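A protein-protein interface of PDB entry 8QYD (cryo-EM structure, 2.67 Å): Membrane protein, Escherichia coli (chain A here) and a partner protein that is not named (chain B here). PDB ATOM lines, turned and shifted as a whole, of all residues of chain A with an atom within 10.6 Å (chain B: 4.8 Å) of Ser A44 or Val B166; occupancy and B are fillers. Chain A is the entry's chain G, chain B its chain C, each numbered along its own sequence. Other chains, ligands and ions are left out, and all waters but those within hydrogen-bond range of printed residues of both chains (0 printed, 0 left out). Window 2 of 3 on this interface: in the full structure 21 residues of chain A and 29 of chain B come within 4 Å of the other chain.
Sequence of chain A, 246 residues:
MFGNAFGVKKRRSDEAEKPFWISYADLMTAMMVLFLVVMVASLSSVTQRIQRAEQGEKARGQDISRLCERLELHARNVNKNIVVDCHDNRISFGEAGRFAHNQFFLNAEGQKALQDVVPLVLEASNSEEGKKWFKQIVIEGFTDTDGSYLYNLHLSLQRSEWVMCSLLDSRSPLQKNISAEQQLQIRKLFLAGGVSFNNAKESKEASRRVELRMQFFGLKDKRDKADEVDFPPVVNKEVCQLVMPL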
ATOM      1  N   LEU A  36     -11.198   5.711   8.389  1.00  0.00           N
ATOM      2  CA  LEU A  36     -10.438   6.385   9.440  1.00  0.00           C
ATOM      3  C   LEU A  36      -9.238   7.135   8.882  1.00  0.00           C
ATOM      4  O   LEU A  36      -9.042   8.322   9.170  1.00  0.00           O
ATOM      5  CB  LEU A  36      -9.970   5.373  10.478  1.00  0.00           C
ATOM      6  CG  LEU A  36      -9.141   6.012  11.591  1.00  0.00           C
ATOM      7  CD1 LEU A  36      -9.923   7.035  12.386  1.00  0.00           C
ATOM      8  CD2 LEU A  36      -8.585   4.937  12.482  1.00  0.00           C
ATOM      9  N   VAL A  37      -8.409   6.449   8.098  1.00  0.00           N
ATOM     10  CA  VAL A  37      -7.170   7.059   7.637  1.00  0.00           C
ATOM     11  C   VAL A  37      -7.450   8.160   6.629  1.00  0.00           C
ATOM     12  O   VAL A  37      -6.728   9.163   6.581  1.00  0.00           O
ATOM     13  CB  VAL A  37      -6.229   5.975   7.084  1.00  0.00           C
ATOM     14  CG1 VAL A  37      -5.034   6.598   6.393  1.00  0.00           C
ATOM     15  CG2 VAL A  37      -5.771   5.086   8.218  1.00  0.00           C
ATOM     16  N   VAL A  38      -8.501   8.018   5.825  1.00  0.00           N
ATOM     17  CA  VAL A  38      -8.847   9.074   4.885  1.00  0.00           C
ATOM     18  C   VAL A  38      -9.354  10.300   5.631  1.00  0.00           C
ATOM     19  O   VAL A  38      -9.039  11.437   5.265  1.00  0.00           O
ATOM     20  CB  VAL A  38      -9.867   8.559   3.856  1.00  0.00           C
ATOM     21  CG1 VAL A  38     -10.534   9.711   3.130  1.00  0.00           C
ATOM     22  CG2 VAL A  38      -9.184   7.635   2.882  1.00  0.00           C
ATOM     23  N   MET A  39     -10.126  10.095   6.703  1.00  0.00           N
ATOM     24  CA  MET A  39     -10.520  11.218   7.546  1.00  0.00           C
ATOM     25  C   MET A  39      -9.306  11.905   8.149  1.00  0.00           C
ATOM     26  O   MET A  39      -9.227  13.137   8.170  1.00  0.00           O
ATOM     27  CB  MET A  39     -11.454  10.742   8.656  1.00  0.00           C
ATOM     28  CG  MET A  39     -11.951  11.859   9.550  1.00  0.00           C
ATOM     29  SD  MET A  39     -13.066  11.266  10.825  1.00  0.00           S
ATOM     30  CE  MET A  39     -11.913  10.408  11.876  1.00  0.00           C
ATOM     31  N   VAL A  40      -8.352  11.121   8.649  1.00  0.00           N
ATOM     32  CA  VAL A  40      -7.162  11.695   9.273  1.00  0.00           C
ATOM     33  C   VAL A  40      -6.374  12.513   8.260  1.00  0.00           C
ATOM     34  O   VAL A  40      -5.970  13.649   8.532  1.00  0.00           O
ATOM     35  CB  VAL A  40      -6.300  10.582   9.894  1.00  0.00           C
ATOM     36  CG1 VAL A  40      -4.901  11.090  10.191  1.00  0.00           C
ATOM     37  CG2 VAL A  40      -6.960  10.054  11.148  1.00  0.00           C
ATOM     38  N   ALA A  41      -6.155  11.949   7.071  1.00  0.00           N
ATOM     39  CA  ALA A  41      -5.408  12.652   6.035  1.00  0.00           C
ATOM     40  C   ALA A  41      -6.130  13.913   5.584  1.00  0.00           C
ATOM     41  O   ALA A  41      -5.508  14.967   5.415  1.00  0.00           O
ATOM     42  CB  ALA A  41      -5.163  11.724   4.847  1.00  0.00           C
ATOM     43  N   SER A  42      -7.447  13.830   5.388  1.00  0.00           N
ATOM     44  CA  SER A  42      -8.201  14.989   4.929  1.00  0.00           C
ATOM     45  C   SER A  42      -8.194  16.102   5.966  1.00  0.00           C
ATOM     46  O   SER A  42      -8.020  17.276   5.619  1.00  0.00           O
ATOM     47  CB  SER A  42      -9.629  14.572   4.593  1.00  0.00           C
ATOM     48  OG  SER A  42      -9.637  13.442   3.743  1.00  0.00           O
ATOM     49  N   LEU A  43      -8.386  15.758   7.240  1.00  0.00           N
ATOM     50  CA  LEU A  43      -8.376  16.772   8.286  1.00  0.00           C
ATOM     51  C   LEU A  43      -6.990  17.378   8.453  1.00  0.00           C
ATOM     52  O   LEU A  43      -6.861  18.587   8.667  1.00  0.00           O
ATOM     53  CB  LEU A  43      -8.867  16.177   9.603  1.00  0.00           C
ATOM     54  CG  LEU A  43     -10.363  15.874   9.660  1.00  0.00           C
ATOM     55  CD1 LEU A  43     -10.744  15.311  11.013  1.00  0.00           C
ATOM     56  CD2 LEU A  43     -11.164  17.121   9.353  1.00  0.00           C
ATOM     57  N   SER A  44      -5.942  16.559   8.360  1.00  0.00           N
ATOM     58  CA  SER A  44      -4.589  17.088   8.438  1.00  0.00           C
ATOM     59  C   SER A  44      -4.228  17.926   7.222  1.00  0.00           C
ATOM     60  O   SER A  44      -3.320  18.760   7.308  1.00  0.00           O
ATOM     61  CB  SER A  44      -3.590  15.944   8.601  1.00  0.00           C
ATOM     62  OG  SER A  44      -3.931  15.136   9.711  1.00  0.00           O
ATOM     63  N   SER A  45      -4.905  17.719   6.094  1.00  0.00           N
ATOM     64  CA  SER A  45      -4.614  18.504   4.902  1.00  0.00           C
ATOM     65  C   SER A  45      -5.354  19.837   4.908  1.00  0.00           C
ATOM     66  O   SER A  45      -4.777  20.870   4.554  1.00  0.00           O
ATOM     67  CB  SER A  45      -4.963  17.701   3.651  1.00  0.00           C
ATOM     68  OG  SER A  45      -4.312  16.444   3.664  1.00  0.00           O
ATOM     69  N   VAL A  46      -6.630  19.839   5.298  1.00  0.00           N
ATOM     70  CA  VAL A  46      -7.396  21.084   5.259  1.00  0.00           C
ATOM     71  C   VAL A  46      -6.854  22.082   6.275  1.00  0.00           C
ATOM     72  O   VAL A  46      -6.867  23.296   6.038  1.00  0.00           O
ATOM     73  CB  VAL A  46      -8.897  20.823   5.476  1.00  0.00           C
ATOM     74  CG1 VAL A  46      -9.505  20.169   4.256  1.00  0.00           C
ATOM     75  CG2 VAL A  46      -9.131  19.988   6.711  1.00  0.00           C
ATOM     76  N   THR A  47      -6.377  21.599   7.419  1.00  0.00           N
ATOM     77  CA  THR A  47      -5.933  22.468   8.497  1.00  0.00           C
ATOM     78  C   THR A  47      -4.420  22.629   8.546  1.00  0.00           C
ATOM     79  O   THR A  47      -3.898  23.149   9.536  1.00  0.00           O
ATOM     80  CB  THR A  47      -6.437  21.950   9.844  1.00  0.00           C
ATOM     81  OG1 THR A  47      -5.638  20.837  10.257  1.00  0.00           O
ATOM     82  CG2 THR A  47      -7.885  21.519   9.746  1.00  0.00           C
ATOM     83  N   GLN A  48      -3.700  22.206   7.503  1.00  0.00           N
ATOM     84  CA  GLN A  48      -2.243  22.268   7.572  1.00  0.00           C
ATOM     85  C   GLN A  48      -1.747  23.707   7.600  1.00  0.00           C
ATOM     86  O   GLN A  48      -0.734  24.002   8.240  1.00  0.00           O
ATOM     87  CB  GLN A  48      -1.605  21.502   6.414  1.00  0.00           C
ATOM     88  CG  GLN A  48      -1.859  22.063   5.034  1.00  0.00           C
ATOM     89  CD  GLN A  48      -1.231  21.205   3.957  1.00  0.00           C
ATOM     90  OE1 GLN A  48      -0.563  20.216   4.250  1.00  0.00           O
ATOM     91  NE2 GLN A  48      -1.435  21.584   2.703  1.00  0.00           N
ATOM     92  N   ARG A  49      -2.436  24.618   6.911  1.00  0.00           N
ATOM     93  CA  ARG A  49      -2.099  26.031   7.048  1.00  0.00           C
ATOM     94  C   ARG A  49      -2.373  26.519   8.462  1.00  0.00           C
ATOM     95  O   ARG A  49      -1.570  27.261   9.039  1.00  0.00           O
ATOM     96  CB  ARG A  49      -2.880  26.865   6.036  1.00  0.00           C
ATOM     97  CG  ARG A  49      -2.448  26.656   4.600  1.00  0.00           C
ATOM     98  CD  ARG A  49      -3.115  27.659   3.680  1.00  0.00           C
ATOM     99  NE  ARG A  49      -3.002  27.272   2.281  1.00  0.00           N
ATOM    100  CZ  ARG A  49      -4.034  26.981   1.501  1.00  0.00           C
ATOM    101  NH1 ARG A  49      -5.275  27.037   1.952  1.00  0.00           N
ATOM    102  NH2 ARG A  49      -3.815  26.629   0.239  1.00  0.00           N
ATOM    103  N   ILE A  50      -3.497  26.098   9.042  1.00  0.00           N
ATOM    104  CA  ILE A  50      -3.815  26.466  10.416  1.00  0.00           C
ATOM    105  C   ILE A  50      -2.820  25.834  11.379  1.00  0.00           C
ATOM    106  O   ILE A  50      -2.390  26.466  12.350  1.00  0.00           O
ATOM    107  CB  ILE A  50      -5.265  26.066  10.742  1.00  0.00           C
ATOM    108  CG1 ILE A  50      -6.207  26.654   9.692  1.00  0.00           C
ATOM    109  CG2 ILE A  50      -5.652  26.538  12.130  1.00  0.00           C
ATOM    110  CD1 ILE A  50      -7.658  26.383   9.951  1.00  0.00           C
ATOM    111  N   GLN A  51      -2.430  24.583  11.123  1.00  0.00           N
ATOM    112  CA  GLN A  51      -1.427  23.934  11.962  1.00  0.00           C
ATOM    113  C   GLN A  51      -0.095  24.669  11.896  1.00  0.00           C
ATOM    114  O   GLN A  51       0.566  24.867  12.919  1.00  0.00           O
ATOM    115  CB  GLN A  51      -1.246  22.473  11.548  1.00  0.00           C
ATOM    116  CG  GLN A  51      -2.440  21.581  11.816  1.00  0.00           C
ATOM    117  CD  GLN A  51      -2.202  20.155  11.368  1.00  0.00           C
ATOM    118  OE1 GLN A  51      -1.161  19.840  10.793  1.00  0.00           O
ATOM    119  NE2 GLN A  51      -3.167  19.282  11.628  1.00  0.00           N
ATOM    120  N   ARG A  52       0.320  25.073  10.695  1.00  0.00           N
ATOM    121  CA  ARG A  52       1.585  25.785  10.549  1.00  0.00           C
ATOM    122  C   ARG A  52       1.534  27.152  11.220  1.00  0.00           C
ATOM    123  O   ARG A  52       2.500  27.567  11.869  1.00  0.00           O
ATOM    124  CB  ARG A  52       1.942  25.923   9.072  1.00  0.00           C
ATOM    125  CG  ARG A  52       3.381  26.323   8.822  1.00  0.00           C
ATOM    126  CD  ARG A  52       3.682  26.414   7.336  1.00  0.00           C
ATOM    127  NE  ARG A  52       3.049  25.341   6.580  1.00  0.00           N
ATOM    128  CZ  ARG A  52       2.230  25.530   5.555  1.00  0.00           C
ATOM    129  NH1 ARG A  52       1.916  26.746   5.137  1.00  0.00           N
ATOM    130  NH2 ARG A  52       1.716  24.475   4.930  1.00  0.00           N
ATOM    131  N   ALA A  53       0.414  27.866  11.078  1.00  0.00           N
ATOM    132  CA  ALA A  53       0.273  29.155  11.747  1.00  0.00           C
ATOM    133  C   ALA A  53       0.297  28.998  13.261  1.00  0.00           C
ATOM    134  O   ALA A  53       0.914  29.803  13.966  1.00  0.00           O
ATOM    135  CB  ALA A  53      -1.015  29.842  11.297  1.00  0.00           C
ATOM    136  N   GLU A  54      -0.369  27.965  13.782  1.00  0.00           N
ATOM    137  CA  GLU A  54      -0.367  27.734  15.223  1.00  0.00           C
ATOM    138  C   GLU A  54       1.020  27.341  15.717  1.00  0.00           C
ATOM    139  O   GLU A  54       1.438  27.755  16.803  1.00  0.00           O
ATOM    140  CB  GLU A  54      -1.401  26.665  15.577  1.00  0.00           C
ATOM    141  CG  GLU A  54      -1.547  26.397  17.063  1.00  0.00           C
ATOM    142  CD  GLU A  54      -2.619  25.368  17.364  1.00  0.00           C
ATOM    143  OE1 GLU A  54      -3.232  24.851  16.405  1.00  0.00           O
ATOM    144  OE2 GLU A  54      -2.853  25.078  18.556  1.00  0.00           O
ATOM    145  N   GLN A  55       1.748  26.543  14.932  1.00  0.00           N
ATOM    146  CA  GLN A  55       3.121  26.202  15.293  1.00  0.00           C
ATOM    147  C   GLN A  55       4.005  27.439  15.316  1.00  0.00           C
ATOM    148  O   GLN A  55       4.833  27.603  16.218  1.00  0.00           O
ATOM    149  CB  GLN A  55       3.684  25.167  14.320  1.00  0.00           C
ATOM    150  CG  GLN A  55       5.119  24.773  14.621  1.00  0.00           C
ATOM    151  CD  GLN A  55       5.903  24.415  13.377  1.00  0.00           C
ATOM    152  OE1 GLN A  55       5.402  24.526  12.259  1.00  0.00           O
ATOM    153  NE2 GLN A  55       7.143  23.983  13.565  1.00  0.00           N
ATOM    154  N   LYS A  58       3.174  29.404  18.437  1.00  0.00           N
ATOM    155  CA  LYS A  58       3.784  28.779  19.606  1.00  0.00           C
ATOM    156  C   LYS A  58       5.286  29.033  19.648  1.00  0.00           C
ATOM    157  O   LYS A  58       5.849  29.277  20.719  1.00  0.00           O
ATOM    158  CB  LYS A  58       3.483  27.280  19.607  1.00  0.00           C
ATOM    159  CG  LYS A  58       4.140  26.502  20.731  1.00  0.00           C
ATOM    160  CD  LYS A  58       3.534  25.113  20.858  1.00  0.00           C
ATOM    161  CE  LYS A  58       3.599  24.353  19.543  1.00  0.00           C
ATOM    162  NZ  LYS A  58       2.435  23.440  19.371  1.00  0.00           N
ATOM    163  N   PHE B 158       2.693   7.541  14.815  1.00  0.00           N
ATOM    164  CA  PHE B 158       2.174   8.828  14.373  1.00  0.00           C
ATOM    165  C   PHE B 158       2.804   9.946  15.192  1.00  0.00           C
ATOM    166  O   PHE B 158       2.761   9.928  16.426  1.00  0.00           O
ATOM    167  CB  PHE B 158       0.653   8.862  14.504  1.00  0.00           C
ATOM    168  CG  PHE B 158       0.024  10.103  13.943  1.00  0.00           C
ATOM    169  CD1 PHE B 158      -0.230  10.215  12.588  1.00  0.00           C
ATOM    170  CD2 PHE B 158      -0.326  11.154  14.771  1.00  0.00           C
ATOM    171  CE1 PHE B 158      -0.811  11.349  12.070  1.00  0.00           C
ATOM    172  CE2 PHE B 158      -0.908  12.292  14.256  1.00  0.00           C
ATOM    173  CZ  PHE B 158      -1.152  12.389  12.904  1.00  0.00           C
ATOM    174  N   ASP B 159       3.387  10.919  14.503  1.00  0.00           N
ATOM    175  CA  ASP B 159       4.126  12.008  15.142  1.00  0.00           C
ATOM    176  C   ASP B 159       3.478  13.338  14.784  1.00  0.00           C
ATOM    177  O   ASP B 159       3.735  13.885  13.697  1.00  0.00           O
ATOM    178  CB  ASP B 159       5.591  11.982  14.709  1.00  0.00           C
ATOM    179  CG  ASP B 159       6.429  13.021  15.418  1.00  0.00           C
ATOM    180  OD1 ASP B 159       5.987  13.541  16.463  1.00  0.00           O
ATOM    181  OD2 ASP B 159       7.540  13.313  14.930  1.00  0.00           O
ATOM    182  N   PRO B 160       2.633  13.892  15.650  1.00  0.00           N
ATOM    183  CA  PRO B 160       1.950  15.158  15.348  1.00  0.00           C
ATOM    184  C   PRO B 160       2.700  16.412  15.773  1.00  0.00           C
ATOM    185  O   PRO B 160       2.092  17.486  15.797  1.00  0.00           O
ATOM    186  CB  PRO B 160       0.659  15.020  16.159  1.00  0.00           C
ATOM    187  CG  PRO B 160       1.088  14.261  17.371  1.00  0.00           C
ATOM    188  CD  PRO B 160       2.211  13.340  16.948  1.00  0.00           C
ATOM    189  N   THR B 162       5.113  18.286  14.454  1.00  0.00           N
ATOM    190  CA  THR B 162       5.462  19.309  13.484  1.00  0.00           C
ATOM    191  C   THR B 162       4.729  19.024  12.180  1.00  0.00           C
ATOM    192  O   THR B 162       4.504  17.859  11.842  1.00  0.00           O
ATOM    193  CB  THR B 162       6.984  19.318  13.272  1.00  0.00           C
ATOM    194  OG1 THR B 162       7.626  19.538  14.532  1.00  0.00           O
ATOM    195  CG2 THR B 162       7.404  20.446  12.377  1.00  0.00           C
ATOM    196  N   PRO B 163       4.312  20.063  11.444  1.00  0.00           N
ATOM    197  CA  PRO B 163       3.482  19.820  10.247  1.00  0.00           C
ATOM    198  C   PRO B 163       4.070  18.857   9.224  1.00  0.00           C
ATOM    199  O   PRO B 163       3.323  18.027   8.689  1.00  0.00           O
ATOM    200  CB  PRO B 163       3.312  21.228   9.672  1.00  0.00           C
ATOM    201  CG  PRO B 163       3.275  22.086  10.880  1.00  0.00           C
ATOM    202  CD  PRO B 163       4.235  21.472  11.870  1.00  0.00           C
ATOM    203  N   GLU B 164       5.372  18.918   8.926  1.00  0.00           N
ATOM    204  CA  GLU B 164       5.910  17.931   7.992  1.00  0.00           C
ATOM    205  C   GLU B 164       6.067  16.568   8.652  1.00  0.00           C
ATOM    206  O   GLU B 164       6.004  15.540   7.967  1.00  0.00           O
ATOM    207  CB  GLU B 164       7.233  18.398   7.377  1.00  0.00           C
ATOM    208  CG  GLU B 164       8.469  18.176   8.223  1.00  0.00           C
ATOM    209  CD  GLU B 164       8.520  19.106   9.405  1.00  0.00           C
ATOM    210  OE1 GLU B 164       7.701  20.047   9.434  1.00  0.00           O
ATOM    211  OE2 GLU B 164       9.371  18.902  10.297  1.00  0.00           O
ATOM    212  N   GLN B 165       6.242  16.531   9.974  1.00  0.00           N
ATOM    213  CA  GLN B 165       6.131  15.264  10.686  1.00  0.00           C
ATOM    214  C   GLN B 165       4.728  14.692  10.543  1.00  0.00           C
ATOM    215  O   GLN B 165       4.559  13.480  10.365  1.00  0.00           O
ATOM    216  CB  GLN B 165       6.490  15.447  12.160  1.00  0.00           C
ATOM    217  CG  GLN B 165       7.974  15.585  12.423  1.00  0.00           C
ATOM    218  CD  GLN B 165       8.741  14.338  12.053  1.00  0.00           C
ATOM    219  OE1 GLN B 165       9.362  14.268  10.994  1.00  0.00           O
ATOM    220  NE2 GLN B 165       8.700  13.340  12.926  1.00  0.00           N
ATOM    221  N   VAL B 166       3.711  15.554  10.602  1.00  0.00           N
ATOM    222  CA  VAL B 166       2.339  15.111  10.377  1.00  0.00           C
ATOM    223  C   VAL B 166       2.181  14.567   8.965  1.00  0.00           C
ATOM    224  O   VAL B 166       1.528  13.539   8.749  1.00  0.00           O
ATOM    225  CB  VAL B 166       1.352  16.262  10.649  1.00  0.00           C
ATOM    226  CG1 VAL B 166      -0.022  15.931  10.098  1.00  0.00           C
ATOM    227  CG2 VAL B 166       1.273  16.554  12.129  1.00  0.00           C
ATOM    228  N   SER B 167       2.765  15.252   7.979  1.00  0.00           N
ATOM    229  CA  SER B 167       2.651  14.803   6.595  1.00  0.00           C
ATOM    230  C   SER B 167       3.299  13.437   6.404  1.00  0.00           C
ATOM    231  O   SER B 167       2.728  12.550   5.758  1.00  0.00           O
ATOM    232  CB  SER B 167       3.281  15.832   5.659  1.00  0.00           C
ATOM    233  OG  SER B 167       2.589  17.065   5.725  1.00  0.00           O
ATOM    234  N   SER B 168       4.495  13.250   6.964  1.00  0.00           N
ATOM    235  CA  SER B 168       5.167  11.960   6.847  1.00  0.00           C
ATOM    236  C   SER B 168       4.395  10.866   7.574  1.00  0.00           C
ATOM    237  O   SER B 168       4.303   9.736   7.083  1.00  0.00           O
ATOM    238  CB  SER B 168       6.594  12.056   7.380  1.00  0.00           C
ATOM    239  OG  SER B 168       6.607  12.141   8.792  1.00  0.00           O
ATOM    240  N   SER B 169       3.831  11.181   8.742  1.00  0.00           N
ATOM    241  CA  SER B 169       3.051  10.191   9.477  1.00  0.00           C
ATOM    242  C   SER B 169       1.796   9.795   8.709  1.00  0.00           C
ATOM    243  O   SER B 169       1.409   8.622   8.696  1.00  0.00           O
ATOM    244  CB  SER B 169       2.688  10.739  10.855  1.00  0.00           C
ATOM    245  OG  SER B 169       3.849  11.087  11.586  1.00  0.00           O
ATOM    246  N   VAL B 170       1.149  10.762   8.059  1.00  0.00           N
ATOM    247  CA  VAL B 170      -0.033  10.465   7.258  1.00  0.00           C
ATOM    248  C   VAL B 170       0.339   9.619   6.046  1.00  0.00           C
ATOM    249  O   VAL B 170      -0.388   8.688   5.674  1.00  0.00           O
ATOM    250  CB  VAL B 170      -0.733  11.775   6.854  1.00  0.00           C
ATOM    251  CG1 VAL B 170      -1.708  11.532   5.728  1.00  0.00           C
ATOM    252  CG2 VAL B 170      -1.440  12.380   8.049  1.00  0.00           C
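The backbone carbonyl oxygen (O) of Ala A41 sits at hydrogen-bond distance from the side-chain hydroxyl (OG) of Ser A45, 2.6 Å away.
O of Val A40 sits at hydrogen-bond distance from OG of Ser A44 (2.8 Å).
The side-chain hydroxyl of Ser B167 lies within hydrogen-bond range of the backbone carbonyl oxygen of Pro B163 (3.2 Å).
Among the printed residues, merely in contact across the chains: Ala A41 with Val B170 (3.6 Å), Ser A44 with Val B166 (3.9 Å), Gln A55 with Thr B162 (3.7 Å) and Gln A55 with Pro B163 (3.3 Å).
Printed residues of chain B within 4 Å of Ala A41: Val B170.
Printed residues of chain B within 4 Å of Ser A44: Val B166.
Of the printed residues of chain A, Thr B162 touches Gln A55 (3.7 Å).
Of chain A, only Gln A55 comes within 4 Å of Pro B163.
Gln B165 touches none of the printed residues of chain A.
No residue of chain A comes within 4 Å of Ser B167.
No residue of chain A comes within 4 Å of Ser B169.
Of the 12 printed residues of chain B, 4 touch a printed residue of chain A.
Hydrophobic or aromatic side chains of chain B that line the printed part of chain A: Pro B163, Val B166 and Val B170.
Along chain B the printed residues that touch a printed residue of chain A span positions 162 to 170.
Of the 21 printed residues of chain A, 3 touch a printed residue of chain B.
Hydrophobic or aromatic side chains of chain A that line the printed part of chain B: Ala A41.
Among the printed residues, no Asp or Glu carboxylate lies within 4 Å of a Lys or Arg side-chain nitrogen of the other chain.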
